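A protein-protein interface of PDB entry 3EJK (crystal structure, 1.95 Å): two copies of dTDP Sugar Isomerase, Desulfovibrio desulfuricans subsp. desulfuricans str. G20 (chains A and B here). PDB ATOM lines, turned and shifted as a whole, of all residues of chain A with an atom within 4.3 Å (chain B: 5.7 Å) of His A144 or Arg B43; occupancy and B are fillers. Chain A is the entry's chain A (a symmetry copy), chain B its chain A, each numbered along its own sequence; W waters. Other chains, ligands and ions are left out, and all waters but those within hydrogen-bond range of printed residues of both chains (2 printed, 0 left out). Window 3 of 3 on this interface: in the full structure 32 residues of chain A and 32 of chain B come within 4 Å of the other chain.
The guanidinium group of Arg B43 lies within salt-bridge range of the side-chain carboxylate of Glu A54, 3.9 Å away. The guanidinium group (NH1) of Arg B43 lies within hydrogen-bond range of the backbone carbonyl oxygen (O) of His A144 (3.3 Å). The backbone NH of Leu B44 is in hydrogen-bond range of the backbone carbonyl oxygen of Gly A53, 3.0 Å away.
The guanidinium group (NE) of Arg B43 is in salt-bridge range of the side-chain carboxylate (OD1) of Asp B45 (2.7 Å). OE1 of Glu A54 is in hydrogen-bond range of N of His A144 (3.1 Å). The backbone NH (N) of Arg B43 is in hydrogen-bond range of the side-chain hydroxyl (OG) of Ser B46 (2.7 Å).
Among the printed residues, merely in contact across the chains: Phe A52 with Phe B49 (3.4 Å), Glu A54 with Leu B42 (3.4 Å), Pro A143 with Arg B43 (3.6 Å), Gly A53 with Arg B43 (3.6 Å), Phe A52 with Leu B44 (3.8 Å), Phe A52 with Leu B42 (3.8 Å) and Phe A52 with Arg B43 (3.8 Å).
His A144 touches just one residue of chain B: Arg B43 (3.3 Å). Of chain A, only Phe A52 (3.8 Å), Gly A53 (3.6 Å), Glu A54 (3.7 Å), Pro A143 (3.6 Å) and His A144 (3.3 Å) come within 4 Å of Arg B43. Of the printed residues of chain A, Leu B42 touches Phe A52 (3.8 Å) and Glu A54 (3.4 Å). Of the printed residues of chain B, Gly A53 touches Arg B43 and Leu B44. Of the printed residues of chain B, Phe A52 touches Leu B42, Arg B43, Leu B44 and Phe B49. Of the printed residues of chain B, Glu A54 touches Leu B42 and Arg B43. The nearest printed residue of chain B that does not touch His A144 is Asp B45 (6.7 Å).
Of the 8 printed residues of chain A, 5 touch a printed residue of chain B. Printed residues of chain A that touch a printed residue of chain B: Phe A52, Gly A53, Glu A54, Pro A143 and His A144. Hydrophobic or aromatic side chains of chain A that line the printed part of chain B: Phe A52 and Pro A143. Of the 7 printed residues of chain B, 4 touch a printed residue of chain A. Hydrophobic or aromatic side chains of chain B that line the printed part of chain A: Leu B44 and Phe B49. Among the printed residues, Asp or Glu carboxylates within 4 Å of a Lys or Arg side-chain nitrogen of the other chain: Glu A54 with Arg B43 (3.9 Å).
No position is printed for both chains.
Water W2 lies within hydrogen-bond range of the side-chain carboxylate of Glu A54, the backbone NH of Met B41 and the backbone NH of Leu B42. Water W1 lies within hydrogen-bond range of the side-chain carboxylate of Glu A54 (2.9 Å) and the guanidinium group of Arg B43 (3.1 Å).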
ATOM      1  N   PHE A  52      26.251 -12.616  -5.574  1.00  0.00           N
ATOM      2  CA  PHE A  52      26.464 -12.780  -7.029  1.00  0.00           C
ATOM      3  C   PHE A  52      26.750 -14.206  -7.472  1.00  0.00           C
ATOM      4  O   PHE A  52      27.777 -14.834  -7.146  1.00  0.00           O
ATOM      5  CB  PHE A  52      27.550 -11.855  -7.590  1.00  0.00           C
ATOM      6  CG  PHE A  52      27.713 -11.976  -9.078  1.00  0.00           C
ATOM      7  CD1 PHE A  52      26.907 -11.263  -9.936  1.00  0.00           C
ATOM      8  CD2 PHE A  52      28.663 -12.817  -9.614  1.00  0.00           C
ATOM      9  CE1 PHE A  52      27.052 -11.389 -11.314  1.00  0.00           C
ATOM     10  CE2 PHE A  52      28.812 -12.946 -10.978  1.00  0.00           C
ATOM     11  CZ  PHE A  52      27.996 -12.235 -11.833  1.00  0.00           C
ATOM     12  N   GLY A  53      25.818 -14.690  -8.256  1.00  0.00           N
ATOM     13  CA  GLY A  53      25.930 -16.020  -8.836  1.00  0.00           C
ATOM     14  C   GLY A  53      26.155 -15.926 -10.329  1.00  0.00           C
ATOM     15  O   GLY A  53      27.147 -16.439 -10.875  1.00  0.00           O
ATOM     16  N   GLU A  54      25.233 -15.235 -10.983  1.00  0.00           N
ATOM     17  CA  GLU A  54      25.298 -15.100 -12.438  1.00  0.00           C
ATOM     18  C   GLU A  54      24.444 -13.960 -12.975  1.00  0.00           C
ATOM     19  O   GLU A  54      23.470 -13.543 -12.366  1.00  0.00           O
ATOM     20  CB  GLU A  54      24.872 -16.446 -13.086  1.00  0.00           C
ATOM     21  CG  GLU A  54      24.796 -16.452 -14.617  1.00  0.00           C
ATOM     22  CD  GLU A  54      24.553 -17.816 -15.230  1.00  0.00           C
ATOM     23  OE1 GLU A  54      24.272 -18.774 -14.459  1.00  0.00           O
ATOM     24  OE2 GLU A  54      24.660 -17.939 -16.492  1.00  0.00           O
ATOM     25  N   MET A  74      17.787 -21.311  -5.668  1.00  0.00           N
ATOM     26  CA  MET A  74      18.069 -20.049  -6.334  1.00  0.00           C
ATOM     27  C   MET A  74      16.942 -19.026  -6.277  1.00  0.00           C
ATOM     28  O   MET A  74      15.760 -19.365  -6.387  1.00  0.00           O
ATOM     29  CB  MET A  74      18.425 -20.310  -7.808  1.00  0.00           C
ATOM     30  CG  MET A  74      18.953 -19.117  -8.534  1.00  0.00           C
ATOM     31  SD  MET A  74      19.096 -19.411 -10.468  1.00  0.00           S
ATOM     32  CE  MET A  74      20.316 -20.891 -10.472  1.00  0.00           C
ATOM     33  N   ILE A 142      22.982 -17.706  -7.270  1.00  0.00           N
ATOM     34  CA  ILE A 142      23.841 -18.863  -7.516  1.00  0.00           C
ATOM     35  C   ILE A 142      23.869 -19.161  -9.004  1.00  0.00           C
ATOM     36  O   ILE A 142      22.899 -18.917  -9.713  1.00  0.00           O
ATOM     37  CB  ILE A 142      23.441 -20.139  -6.735  1.00  0.00           C
ATOM     38  CG1 ILE A 142      22.046 -20.597  -7.103  1.00  0.00           C
ATOM     39  CG2 ILE A 142      23.518 -19.885  -5.241  1.00  0.00           C
ATOM     40  CD1 ILE A 142      21.648 -21.897  -6.385  1.00  0.00           C
ATOM     41  N   PRO A 143      24.988 -19.685  -9.488  1.00  0.00           N
ATOM     42  CA  PRO A 143      25.025 -19.958 -10.907  1.00  0.00           C
ATOM     43  C   PRO A 143      24.171 -21.159 -11.273  1.00  0.00           C
ATOM     44  O   PRO A 143      23.769 -21.950 -10.424  1.00  0.00           O
ATOM     45  CB  PRO A 143      26.500 -20.238 -11.166  1.00  0.00           C
ATOM     46  CG  PRO A 143      27.029 -20.710  -9.891  1.00  0.00           C
ATOM     47  CD  PRO A 143      26.236 -20.066  -8.809  1.00  0.00           C
ATOM     48  N   HIS A 144      23.864 -21.237 -12.551  1.00  0.00           N
ATOM     49  CA  HIS A 144      23.076 -22.351 -13.051  1.00  0.00           C
ATOM     50  C   HIS A 144      23.779 -23.673 -12.870  1.00  0.00           C
ATOM     51  O   HIS A 144      24.939 -23.819 -13.192  1.00  0.00           O
ATOM     52  CB  HIS A 144      22.753 -22.192 -14.525  1.00  0.00           C
ATOM     53  CG  HIS A 144      21.975 -23.341 -15.069  1.00  0.00           C
ATOM     54  ND1 HIS A 144      20.603 -23.414 -14.965  1.00  0.00           N
ATOM     55  CD2 HIS A 144      22.376 -24.490 -15.665  1.00  0.00           C
ATOM     56  CE1 HIS A 144      20.189 -24.546 -15.505  1.00  0.00           C
ATOM     57  NE2 HIS A 144      21.244 -25.221 -15.929  1.00  0.00           N
ATOM     58  N   ARG A 145      23.043 -24.651 -12.366  1.00  0.00           N
ATOM     59  CA  ARG A 145      23.575 -26.001 -12.203  1.00  0.00           C
ATOM     60  C   ARG A 145      22.538 -27.081 -12.444  1.00  0.00           C
ATOM     61  O   ARG A 145      21.393 -26.996 -11.984  1.00  0.00           O
ATOM     62  CB  ARG A 145      24.191 -26.186 -10.819  1.00  0.00           C
ATOM     63  CG  ARG A 145      25.408 -25.320 -10.573  1.00  0.00           C
ATOM     64  CD  ARG A 145      26.085 -25.735  -9.278  1.00  0.00           C
ATOM     65  NE  ARG A 145      27.180 -24.847  -8.902  1.00  0.00           N
ATOM     66  CZ  ARG A 145      27.018 -23.720  -8.213  1.00  0.00           C
ATOM     67  NH1 ARG A 145      25.801 -23.328  -7.859  1.00  0.00           N
ATOM     68  NH2 ARG A 145      28.072 -22.970  -7.898  1.00  0.00           N
ATOM     69  N   MET B  41      26.498 -13.877 -19.971  1.00  0.00           N
ATOM     70  CA  MET B  41      27.349 -12.727 -19.728  1.00  0.00           C
ATOM     71  C   MET B  41      28.497 -13.043 -18.762  1.00  0.00           C
ATOM     72  O   MET B  41      29.684 -13.011 -19.132  1.00  0.00           O
ATOM     73  CB  MET B  41      26.565 -11.523 -19.214  1.00  0.00           C
ATOM     74  CG  MET B  41      27.455 -10.317 -19.195  1.00  0.00           C
ATOM     75  SD  MET B  41      26.620  -8.695 -18.597  1.00  0.00           S
ATOM     76  CE  MET B  41      28.171  -7.438 -18.799  1.00  0.00           C
ATOM     77  N   LEU B  42      28.129 -13.358 -17.526  1.00  0.00           N
ATOM     78  CA  LEU B  42      29.139 -13.608 -16.500  1.00  0.00           C
ATOM     79  C   LEU B  42      28.640 -14.467 -15.361  1.00  0.00           C
ATOM     80  O   LEU B  42      27.491 -14.371 -14.934  1.00  0.00           O
ATOM     81  CB  LEU B  42      29.601 -12.248 -15.945  1.00  0.00           C
ATOM     82  CG  LEU B  42      30.943 -12.045 -15.258  1.00  0.00           C
ATOM     83  CD1 LEU B  42      32.112 -12.445 -16.171  1.00  0.00           C
ATOM     84  CD2 LEU B  42      31.003 -10.562 -14.841  1.00  0.00           C
ATOM     85  N   ARG B  43      29.534 -15.332 -14.914  1.00  0.00           N
ATOM     86  CA  ARG B  43      29.310 -16.192 -13.761  1.00  0.00           C
ATOM     87  C   ARG B  43      30.396 -15.945 -12.729  1.00  0.00           C
ATOM     88  O   ARG B  43      31.462 -15.405 -13.031  1.00  0.00           O
ATOM     89  CB  ARG B  43      29.364 -17.670 -14.124  1.00  0.00           C
ATOM     90  CG  ARG B  43      28.164 -18.221 -14.812  1.00  0.00           C
ATOM     91  CD  ARG B  43      28.562 -19.533 -15.431  1.00  0.00           C
ATOM     92  NE  ARG B  43      28.980 -20.544 -14.459  1.00  0.00           N
ATOM     93  CZ  ARG B  43      28.188 -21.535 -14.046  1.00  0.00           C
ATOM     94  NH1 ARG B  43      26.959 -21.620 -14.512  1.00  0.00           N
ATOM     95  NH2 ARG B  43      28.609 -22.443 -13.172  1.00  0.00           N
ATOM     96  N   LEU B  44      30.124 -16.436 -11.529  1.00  0.00           N
ATOM     97  CA  LEU B  44      31.042 -16.298 -10.388  1.00  0.00           C
ATOM     98  C   LEU B  44      32.342 -17.049 -10.628  1.00  0.00           C
ATOM     99  O   LEU B  44      33.399 -16.685 -10.132  1.00  0.00           O
ATOM    100  CB  LEU B  44      30.387 -16.819  -9.101  1.00  0.00           C
ATOM    101  CG  LEU B  44      31.291 -16.939  -7.880  1.00  0.00           C
ATOM    102  CD1 LEU B  44      31.940 -15.610  -7.518  1.00  0.00           C
ATOM    103  CD2 LEU B  44      30.485 -17.490  -6.720  1.00  0.00           C
ATOM    104  N   ASP B  45      32.232 -18.107 -11.392  1.00  0.00           N
ATOM    105  CA  ASP B  45      33.378 -18.954 -11.697  1.00  0.00           C
ATOM    106  C   ASP B  45      33.961 -18.631 -13.058  1.00  0.00           C
ATOM    107  O   ASP B  45      34.932 -19.229 -13.485  1.00  0.00           O
ATOM    108  CB  ASP B  45      33.031 -20.436 -11.560  1.00  0.00           C
ATOM    109  CG  ASP B  45      31.727 -20.803 -12.234  1.00  0.00           C
ATOM    110  OD1 ASP B  45      31.251 -20.029 -13.090  1.00  0.00           O
ATOM    111  OD2 ASP B  45      31.171 -21.863 -11.891  1.00  0.00           O
ATOM    112  N   SER B  46      33.389 -17.634 -13.719  1.00  0.00           N
ATOM    113  CA  SER B  46      33.877 -17.246 -15.053  1.00  0.00           C
ATOM    114  C   SER B  46      35.325 -16.825 -14.926  1.00  0.00           C
ATOM    115  O   SER B  46      35.690 -16.134 -13.981  1.00  0.00           O
ATOM    116  CB  SER B  46      33.093 -16.077 -15.666  1.00  0.00           C
ATOM    117  OG  SER B  46      31.762 -16.431 -15.995  1.00  0.00           O
ATOM    118  N   PHE B  49      35.533 -13.166 -14.421  1.00  0.00           N
ATOM    119  CA  PHE B  49      34.932 -12.532 -13.246  1.00  0.00           C
ATOM    120  C   PHE B  49      35.992 -12.299 -12.202  1.00  0.00           C
ATOM    121  O   PHE B  49      36.842 -13.160 -11.948  1.00  0.00           O
ATOM    122  CB  PHE B  49      33.790 -13.372 -12.664  1.00  0.00           C
ATOM    123  CG  PHE B  49      33.162 -12.776 -11.425  1.00  0.00           C
ATOM    124  CD1 PHE B  49      32.252 -11.736 -11.517  1.00  0.00           C
ATOM    125  CD2 PHE B  49      33.470 -13.272 -10.170  1.00  0.00           C
ATOM    126  CE1 PHE B  49      31.664 -11.197 -10.375  1.00  0.00           C
ATOM    127  CE2 PHE B  49      32.897 -12.739  -9.029  1.00  0.00           C
ATOM    128  CZ  PHE B  49      31.990 -11.702  -9.131  1.00  0.00           C
HETATM  129  O   HOH W   1      25.720 -20.516 -17.162  1.00  0.00           O
HETATM  130  O   HOH W   2      25.905 -16.013 -17.897  1.00  0.00           O
